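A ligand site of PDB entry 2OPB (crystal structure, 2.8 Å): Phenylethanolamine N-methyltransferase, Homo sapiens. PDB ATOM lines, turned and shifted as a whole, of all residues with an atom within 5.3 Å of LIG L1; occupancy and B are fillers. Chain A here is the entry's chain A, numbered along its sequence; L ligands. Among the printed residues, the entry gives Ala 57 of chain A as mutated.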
ATOM      1  N   TYR A  35      18.439  10.191 -33.067  1.00  0.00           N
ATOM      2  CA  TYR A  35      18.495   9.565 -31.763  1.00  0.00           C
ATOM      3  C   TYR A  35      17.240   9.965 -30.986  1.00  0.00           C
ATOM      4  O   TYR A  35      16.547   9.133 -30.395  1.00  0.00           O
ATOM      5  CB  TYR A  35      19.727  10.033 -30.996  1.00  0.00           C
ATOM      6  CG  TYR A  35      19.746   9.538 -29.575  1.00  0.00           C
ATOM      7  CD1 TYR A  35      20.020   8.199 -29.284  1.00  0.00           C
ATOM      8  CD2 TYR A  35      19.484  10.396 -28.506  1.00  0.00           C
ATOM      9  CE1 TYR A  35      20.039   7.733 -27.981  1.00  0.00           C
ATOM     10  CE2 TYR A  35      19.499   9.942 -27.192  1.00  0.00           C
ATOM     11  CZ  TYR A  35      19.775   8.607 -26.940  1.00  0.00           C
ATOM     12  OH  TYR A  35      19.819   8.165 -25.653  1.00  0.00           O
ATOM     13  N   ASN A  39      13.947   7.691 -29.720  1.00  0.00           N
ATOM     14  CA  ASN A  39      13.636   7.468 -28.318  1.00  0.00           C
ATOM     15  C   ASN A  39      12.725   8.456 -27.572  1.00  0.00           C
ATOM     16  O   ASN A  39      12.132   8.081 -26.555  1.00  0.00           O
ATOM     17  CB  ASN A  39      14.969   7.322 -27.556  1.00  0.00           C
ATOM     18  CG  ASN A  39      15.857   6.243 -28.144  1.00  0.00           C
ATOM     19  OD1 ASN A  39      15.588   5.048 -27.986  1.00  0.00           O
ATOM     20  ND2 ASN A  39      16.907   6.654 -28.824  1.00  0.00           N
ATOM     21  N   TYR A  40      12.603   9.688 -28.033  1.00  0.00           N
ATOM     22  CA  TYR A  40      11.770  10.632 -27.299  1.00  0.00           C
ATOM     23  C   TYR A  40      10.531  11.143 -27.991  1.00  0.00           C
ATOM     24  O   TYR A  40       9.864  12.027 -27.480  1.00  0.00           O
ATOM     25  CB  TYR A  40      12.625  11.789 -26.812  1.00  0.00           C
ATOM     26  CG  TYR A  40      13.742  11.298 -25.951  1.00  0.00           C
ATOM     27  CD1 TYR A  40      14.978  10.933 -26.513  1.00  0.00           C
ATOM     28  CD2 TYR A  40      13.556  11.113 -24.580  1.00  0.00           C
ATOM     29  CE1 TYR A  40      15.993  10.406 -25.712  1.00  0.00           C
ATOM     30  CE2 TYR A  40      14.565  10.577 -23.781  1.00  0.00           C
ATOM     31  CZ  TYR A  40      15.780  10.237 -24.350  1.00  0.00           C
ATOM     32  OH  TYR A  40      16.765   9.737 -23.537  1.00  0.00           O
ATOM     33  N   ARG A  44       7.652   5.859 -27.350  1.00  0.00           N
ATOM     34  CA  ARG A  44       8.378   5.974 -26.104  1.00  0.00           C
ATOM     35  C   ARG A  44       8.234   7.372 -25.515  1.00  0.00           C
ATOM     36  O   ARG A  44       8.388   7.576 -24.312  1.00  0.00           O
ATOM     37  CB  ARG A  44       9.860   5.661 -26.326  1.00  0.00           C
ATOM     38  CG  ARG A  44      10.110   4.215 -26.695  1.00  0.00           C
ATOM     39  CD  ARG A  44      11.581   3.959 -26.869  1.00  0.00           C
ATOM     40  NE  ARG A  44      11.824   2.560 -27.212  1.00  0.00           N
ATOM     41  CZ  ARG A  44      13.042   2.040 -27.371  1.00  0.00           C
ATOM     42  NH1 ARG A  44      14.114   2.808 -27.207  1.00  0.00           N
ATOM     43  NH2 ARG A  44      13.192   0.759 -27.682  1.00  0.00           N
ATOM     44  N   GLY A  45       7.909   8.329 -26.384  1.00  0.00           N
ATOM     45  CA  GLY A  45       7.746   9.702 -25.940  1.00  0.00           C
ATOM     46  C   GLY A  45       6.351  10.095 -25.503  1.00  0.00           C
ATOM     47  O   GLY A  45       6.164  11.177 -24.967  1.00  0.00           O
ATOM     48  N   VAL A  53       7.311   4.385 -20.238  1.00  0.00           N
ATOM     49  CA  VAL A  53       8.642   4.511 -19.653  1.00  0.00           C
ATOM     50  C   VAL A  53       8.958   5.989 -19.408  1.00  0.00           C
ATOM     51  O   VAL A  53       9.768   6.335 -18.542  1.00  0.00           O
ATOM     52  CB  VAL A  53       9.711   3.894 -20.597  1.00  0.00           C
ATOM     53  CG1 VAL A  53       9.791   4.715 -21.860  1.00  0.00           C
ATOM     54  CG2 VAL A  53      11.078   3.832 -19.903  1.00  0.00           C
ATOM     55  N   GLY A  54       8.330   6.871 -20.167  1.00  0.00           N
ATOM     56  CA  GLY A  54       8.567   8.294 -19.953  1.00  0.00           C
ATOM     57  C   GLY A  54       8.119   8.661 -18.551  1.00  0.00           C
ATOM     58  O   GLY A  54       8.897   9.135 -17.721  1.00  0.00           O
ATOM     59  N   ALA A  57      10.294   7.121 -15.694  1.00  0.00           N
ATOM     60  CA  ALA A  57      11.607   7.741 -15.459  1.00  0.00           C
ATOM     61  C   ALA A  57      11.481   9.106 -14.803  1.00  0.00           C
ATOM     62  O   ALA A  57      12.192   9.414 -13.846  1.00  0.00           O
ATOM     63  CB  ALA A  57      12.357   7.861 -16.765  1.00  0.00           C
ATOM     64  N   TYR A  85      15.541  16.165 -20.363  1.00  0.00           N
ATOM     65  CA  TYR A  85      14.566  15.549 -19.453  1.00  0.00           C
ATOM     66  C   TYR A  85      15.202  15.056 -18.149  1.00  0.00           C
ATOM     67  O   TYR A  85      14.616  15.158 -17.080  1.00  0.00           O
ATOM     68  CB  TYR A  85      13.857  14.379 -20.169  1.00  0.00           C
ATOM     69  CG  TYR A  85      14.685  13.105 -20.249  1.00  0.00           C
ATOM     70  CD1 TYR A  85      14.702  12.202 -19.195  1.00  0.00           C
ATOM     71  CD2 TYR A  85      15.506  12.851 -21.348  1.00  0.00           C
ATOM     72  CE1 TYR A  85      15.523  11.076 -19.226  1.00  0.00           C
ATOM     73  CE2 TYR A  85      16.327  11.726 -21.390  1.00  0.00           C
ATOM     74  CZ  TYR A  85      16.328  10.853 -20.322  1.00  0.00           C
ATOM     75  OH  TYR A  85      17.151   9.770 -20.337  1.00  0.00           O
ATOM     76  N   TYR A 126       7.743  17.244 -21.916  1.00  0.00           N
ATOM     77  CA  TYR A 126       8.503  16.655 -20.831  1.00  0.00           C
ATOM     78  C   TYR A 126       8.499  17.638 -19.644  1.00  0.00           C
ATOM     79  O   TYR A 126       8.299  17.239 -18.493  1.00  0.00           O
ATOM     80  CB  TYR A 126       9.926  16.334 -21.308  1.00  0.00           C
ATOM     81  CG  TYR A 126      10.001  15.117 -22.220  1.00  0.00           C
ATOM     82  CD1 TYR A 126       9.460  15.148 -23.510  1.00  0.00           C
ATOM     83  CD2 TYR A 126      10.573  13.910 -21.777  1.00  0.00           C
ATOM     84  CE1 TYR A 126       9.492  14.013 -24.341  1.00  0.00           C
ATOM     85  CE2 TYR A 126      10.605  12.774 -22.599  1.00  0.00           C
ATOM     86  CZ  TYR A 126      10.056  12.832 -23.886  1.00  0.00           C
ATOM     87  OH  TYR A 126      10.086  11.733 -24.713  1.00  0.00           O
ATOM     88  N   PHE A 182      21.899   6.568 -19.719  1.00  0.00           N
ATOM     89  CA  PHE A 182      22.240   5.774 -20.888  1.00  0.00           C
ATOM     90  C   PHE A 182      23.608   6.092 -21.466  1.00  0.00           C
ATOM     91  O   PHE A 182      23.794   6.022 -22.689  1.00  0.00           O
ATOM     92  CB  PHE A 182      21.181   5.976 -21.975  1.00  0.00           C
ATOM     93  CG  PHE A 182      19.787   5.681 -21.525  1.00  0.00           C
ATOM     94  CD1 PHE A 182      18.850   6.700 -21.422  1.00  0.00           C
ATOM     95  CD2 PHE A 182      19.404   4.379 -21.225  1.00  0.00           C
ATOM     96  CE1 PHE A 182      17.544   6.422 -21.027  1.00  0.00           C
ATOM     97  CE2 PHE A 182      18.093   4.091 -20.832  1.00  0.00           C
ATOM     98  CZ  PHE A 182      17.161   5.120 -20.737  1.00  0.00           C
ATOM     99  N   ALA A 186      26.506   2.446 -23.031  1.00  0.00           N
ATOM    100  CA  ALA A 186      26.506   2.712 -24.469  1.00  0.00           C
ATOM    101  C   ALA A 186      27.864   3.090 -25.021  1.00  0.00           C
ATOM    102  O   ALA A 186      28.050   3.203 -26.230  1.00  0.00           O
ATOM    103  CB  ALA A 186      25.488   3.795 -24.785  1.00  0.00           C
ATOM    104  N   ALA A 216      20.143   1.353 -19.700  1.00  0.00           N
ATOM    105  CA  ALA A 216      19.509   0.253 -20.393  1.00  0.00           C
ATOM    106  C   ALA A 216      19.980  -1.116 -19.885  1.00  0.00           C
ATOM    107  O   ALA A 216      21.181  -1.396 -19.801  1.00  0.00           O
ATOM    108  CB  ALA A 216      19.795   0.377 -21.889  1.00  0.00           C
ATOM    109  N   GLU A 219      20.870  -4.585 -23.012  1.00  0.00           N
ATOM    110  CA  GLU A 219      20.801  -4.061 -24.360  1.00  0.00           C
ATOM    111  C   GLU A 219      22.161  -4.263 -24.996  1.00  0.00           C
ATOM    112  O   GLU A 219      23.173  -4.261 -24.308  1.00  0.00           O
ATOM    113  CB  GLU A 219      20.435  -2.577 -24.334  1.00  0.00           C
ATOM    114  CG  GLU A 219      20.474  -1.904 -25.689  1.00  0.00           C
ATOM    115  CD  GLU A 219      20.212  -0.424 -25.578  1.00  0.00           C
ATOM    116  OE1 GLU A 219      19.096   0.038 -25.877  1.00  0.00           O
ATOM    117  OE2 GLU A 219      21.142   0.283 -25.166  1.00  0.00           O
ATOM    118  N   TYR A 222      21.836  -0.132 -30.590  1.00  0.00           N
ATOM    119  CA  TYR A 222      20.763   0.826 -30.793  1.00  0.00           C
ATOM    120  C   TYR A 222      21.173   1.698 -31.955  1.00  0.00           C
ATOM    121  O   TYR A 222      22.353   2.024 -32.106  1.00  0.00           O
ATOM    122  CB  TYR A 222      20.548   1.675 -29.541  1.00  0.00           C
ATOM    123  CG  TYR A 222      21.620   2.720 -29.291  1.00  0.00           C
ATOM    124  CD1 TYR A 222      21.386   4.071 -29.580  1.00  0.00           C
ATOM    125  CD2 TYR A 222      22.845   2.376 -28.730  1.00  0.00           C
ATOM    126  CE1 TYR A 222      22.346   5.039 -29.314  1.00  0.00           C
ATOM    127  CE2 TYR A 222      23.808   3.331 -28.466  1.00  0.00           C
ATOM    128  CZ  TYR A 222      23.560   4.654 -28.749  1.00  0.00           C
ATOM    129  OH  TYR A 222      24.490   5.610 -28.446  1.00  0.00           O
ATOM    130  N   VAL A 231      26.382  -1.943 -27.520  1.00  0.00           N
ATOM    131  CA  VAL A 231      26.019  -1.667 -26.146  1.00  0.00           C
ATOM    132  C   VAL A 231      26.407  -2.895 -25.341  1.00  0.00           C
ATOM    133  O   VAL A 231      26.467  -3.998 -25.875  1.00  0.00           O
ATOM    134  CB  VAL A 231      24.482  -1.425 -26.017  1.00  0.00           C
ATOM    135  CG1 VAL A 231      24.084  -1.175 -24.568  1.00  0.00           C
ATOM    136  CG2 VAL A 231      24.071  -0.253 -26.901  1.00  0.00           C
ATOM    137  N   MET A 258      10.658  -3.014 -20.362  1.00  0.00           N
ATOM    138  CA  MET A 258      10.151  -2.400 -21.575  1.00  0.00           C
ATOM    139  C   MET A 258       9.010  -3.205 -22.150  1.00  0.00           C
ATOM    140  O   MET A 258       9.185  -4.358 -22.484  1.00  0.00           O
ATOM    141  CB  MET A 258      11.263  -2.285 -22.605  1.00  0.00           C
ATOM    142  CG  MET A 258      11.004  -1.203 -23.626  1.00  0.00           C
ATOM    143  SD  MET A 258      11.010   0.472 -22.904  1.00  0.00           S
ATOM    144  CE  MET A 258      12.586   1.053 -23.470  1.00  0.00           C
ATOM    145  N   ASP A 267      16.486  -0.366 -31.264  1.00  0.00           N
ATOM    146  CA  ASP A 267      17.418  -1.045 -30.375  1.00  0.00           C
ATOM    147  C   ASP A 267      16.809  -2.350 -29.903  1.00  0.00           C
ATOM    148  O   ASP A 267      15.737  -2.733 -30.381  1.00  0.00           O
ATOM    149  CB  ASP A 267      17.803  -0.169 -29.187  1.00  0.00           C
ATOM    150  CG  ASP A 267      16.615   0.370 -28.429  1.00  0.00           C
ATOM    151  OD1 ASP A 267      15.715  -0.428 -28.054  1.00  0.00           O
ATOM    152  OD2 ASP A 267      16.599   1.609 -28.188  1.00  0.00           O
ATOM    153  N   VAL A 269      16.898  -3.106 -26.354  1.00  0.00           N
ATOM    154  CA  VAL A 269      16.826  -2.950 -24.904  1.00  0.00           C
ATOM    155  C   VAL A 269      15.685  -3.823 -24.277  1.00  0.00           C
ATOM    156  O   VAL A 269      14.625  -3.995 -24.888  1.00  0.00           O
ATOM    157  CB  VAL A 269      16.616  -1.431 -24.555  1.00  0.00           C
ATOM    158  CG1 VAL A 269      15.286  -0.948 -25.102  1.00  0.00           C
ATOM    159  CG2 VAL A 269      16.694  -1.218 -23.050  1.00  0.00           C
ATOM    160  N   VAL A 272      14.724  -0.846 -18.280  1.00  0.00           N
ATOM    161  CA  VAL A 272      15.539   0.311 -17.945  1.00  0.00           C
ATOM    162  C   VAL A 272      15.726   0.392 -16.443  1.00  0.00           C
ATOM    163  O   VAL A 272      14.804   0.081 -15.674  1.00  0.00           O
ATOM    164  CB  VAL A 272      14.885   1.619 -18.438  1.00  0.00           C
ATOM    165  CG1 VAL A 272      15.646   2.812 -17.909  1.00  0.00           C
ATOM    166  CG2 VAL A 272      14.880   1.658 -19.967  1.00  0.00           C
HETATM  167  C1  LIG L   1      13.901   7.033 -21.370  1.00  0.00           C
HETATM  168  C2  LIG L   1      13.178   8.040 -20.472  1.00  0.00           C
HETATM  169  S1  LIG L   1      12.434   9.305 -21.560  1.00  0.00           S
HETATM  170  C3  LIG L   1      11.525   8.382 -22.837  1.00  0.00           C
HETATM  171  C4  LIG L   1      12.503   7.339 -23.396  1.00  0.00           C
HETATM  172  N1  LIG L   1      12.945   6.435 -22.325  1.00  0.00           N
HETATM  173  S2  LIG L   1      13.571   5.103 -23.016  1.00  0.00           S
HETATM  174  O1  LIG L   1      13.574   4.077 -22.019  1.00  0.00           O
HETATM  175  O2  LIG L   1      12.655   4.705 -24.135  1.00  0.00           O
HETATM  176  C5  LIG L   1      15.183   5.228 -23.701  1.00  0.00           C
HETATM  177  C6  LIG L   1      15.770   4.056 -24.152  1.00  0.00           C
HETATM  178  C7  LIG L   1      17.054   4.082 -24.711  1.00  0.00           C
HETATM  179  C8  LIG L   1      17.682   2.759 -25.169  1.00  0.00           C
HETATM  180  N2  LIG L   1      18.887   2.986 -25.988  1.00  0.00           N
HETATM  181  C9  LIG L   1      19.781   3.916 -25.306  1.00  0.00           C
HETATM  182  C10 LIG L   1      21.163   3.938 -25.974  1.00  0.00           C
HETATM  183  F1  LIG L   1      21.850   2.761 -25.704  1.00  0.00           F
HETATM  184  C11 LIG L   1      19.162   5.322 -25.352  1.00  0.00           C
HETATM  185  C12 LIG L   1      17.737   5.273 -24.801  1.00  0.00           C
HETATM  186  C13 LIG L   1      17.139   6.464 -24.349  1.00  0.00           C
HETATM  187  C14 LIG L   1      15.868   6.443 -23.798  1.00  0.00           C
HETATM  188  N1  LG2 L   2      22.068  10.846 -21.883  1.00  0.00           N
HETATM  189  C1  LG2 L   2      21.225  11.009 -23.067  1.00  0.00           C
HETATM  190  C2  LG2 L   2      21.932  10.400 -24.308  1.00  0.00           C
HETATM  191  C3  LG2 L   2      22.443   8.959 -24.161  1.00  0.00           C
HETATM  192  S1  LG2 L   2      23.152   8.287 -25.682  1.00  0.00           S
HETATM  193  C4  LG2 L   2      19.850  10.373 -22.813  1.00  0.00           C
HETATM  194  O1  LG2 L   2      19.179   9.892 -23.770  1.00  0.00           O
HETATM  195  O2  LG2 L   2      19.444  10.400 -21.625  1.00  0.00           O
HETATM  196  C5  LG2 L   2      24.900   8.017 -25.201  1.00  0.00           C
HETATM  197  C6  LG2 L   2      25.681   9.316 -25.223  1.00  0.00           C
HETATM  198  O3  LG2 L   2      27.054   9.137 -24.775  1.00  0.00           O
HETATM  199  C7  LG2 L   2      25.749  10.061 -26.546  1.00  0.00           C
HETATM  200  O4  LG2 L   2      25.293  11.395 -26.352  1.00  0.00           O
HETATM  201  C8  LG2 L   2      27.224   9.986 -26.929  1.00  0.00           C
HETATM  202  O5  LG2 L   2      27.704  11.079 -27.666  1.00  0.00           O
HETATM  203  C9  LG2 L   2      27.888   9.965 -25.552  1.00  0.00           C
HETATM  204  N2  LG2 L   2      29.266   9.453 -25.532  1.00  0.00           N
HETATM  205  C10 LG2 L   2      29.991   8.741 -26.543  1.00  0.00           C
HETATM  206  N3  LG2 L   2      31.229   8.470 -26.204  1.00  0.00           N
HETATM  207  C11 LG2 L   2      31.332   9.006 -24.929  1.00  0.00           C
HETATM  208  C12 LG2 L   2      32.451   9.025 -24.064  1.00  0.00           C
HETATM  209  N4  LG2 L   2      33.629   8.504 -24.375  1.00  0.00           N
HETATM  210  N5  LG2 L   2      32.295   9.614 -22.853  1.00  0.00           N
HETATM  211  C13 LG2 L   2      31.082  10.156 -22.550  1.00  0.00           C
HETATM  212  N6  LG2 L   2      29.958  10.203 -23.297  1.00  0.00           N
HETATM  213  C14 LG2 L   2      30.154   9.601 -24.497  1.00  0.00           C
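OH of Tyr 35 touches C11 of LIG L1 (2.9 Å). O of Asn 39 touches C4 of LIG L1, at 3.3 Å. CE2 of Tyr 40 touches S1 of LIG L1, at 3.3 Å. CD of Arg 44 touches O2 of LIG L1, 3.0 Å away. Val 53 touches LIG L1. Ala 57 touches LIG L1 (CB to C2, 3.8 Å). Phe 182 touches LIG L1. Ala 186 touches LIG L1 (CB to F1, 3.9 Å). Tyr 222 touches LIG L1 (CD2 to F1, 3.2 Å). Val 231 touches LIG L1. Met 258 touches LIG L1 (CE to O1, 3.5 Å). Val 272 touches LIG L1 (CG2 to O1, 3.4 Å). Hydrophobic or aromatic side chains within 4 Å of LIG L1: Tyr 35, Tyr 40, Val 53, Ala 57, Phe 182, Ala 186, Tyr 222, Val 231, Met 258 and Val 272. Within 4 Å of LIG L1: Tyr 35, Asn 39, Tyr 40, Arg 44, Val 53, Ala 57, Phe 182, Ala 186, Glu 219, Tyr 222, Val 231, Met 258, Asp 267 and Val 272. Along chain A the residues within 4 Å of LIG L1 span positions 35 to 272.
A nitrogen (N2) of LIG L1 lies within salt-bridge range of the side-chain carboxylate (OE1) of Glu 219 (3.0 Å). The side-chain carboxylate of Asp 267 lies within salt-bridge range of a nitrogen (N2) of LIG L1 (3.5 Å). The side-chain hydroxyl (OH) of Tyr 35 is in hydrogen-bond range of an oxygen (O1) of LG2 L2 (2.6 Å). The side-chain hydroxyl (OH) of Tyr 40 lies within hydrogen-bond range of an oxygen (O1) of LG2 L2 (2.4 Å). OH of Tyr 85 is in hydrogen-bond range of O2 of LG2 L2, 2.7 Å away.
O of Tyr 35 lies within hydrogen-bond range of ND2 of Asn 39. The guanidinium group (NH1) of Arg 44 lies within hydrogen-bond range of the side-chain amide oxygen (OD1) of Asn 39, at 2.8 Å. The guanidinium group (NH2) of Arg 44 is in salt-bridge range of the side-chain carboxylate (OD1) of Asp 267 (2.8 Å). The side-chain hydroxyl (OH) of Tyr 85 lies close to the side-chain hydroxyl (OH) of Tyr 40 (3.2 Å). O of Tyr 40 is in hydrogen-bond range of OH of Tyr 126 (2.8 Å). The side-chain carboxylate (OD1) of Asp 267 sits close to the backbone NH (N) of Val 269 (3.4 Å).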
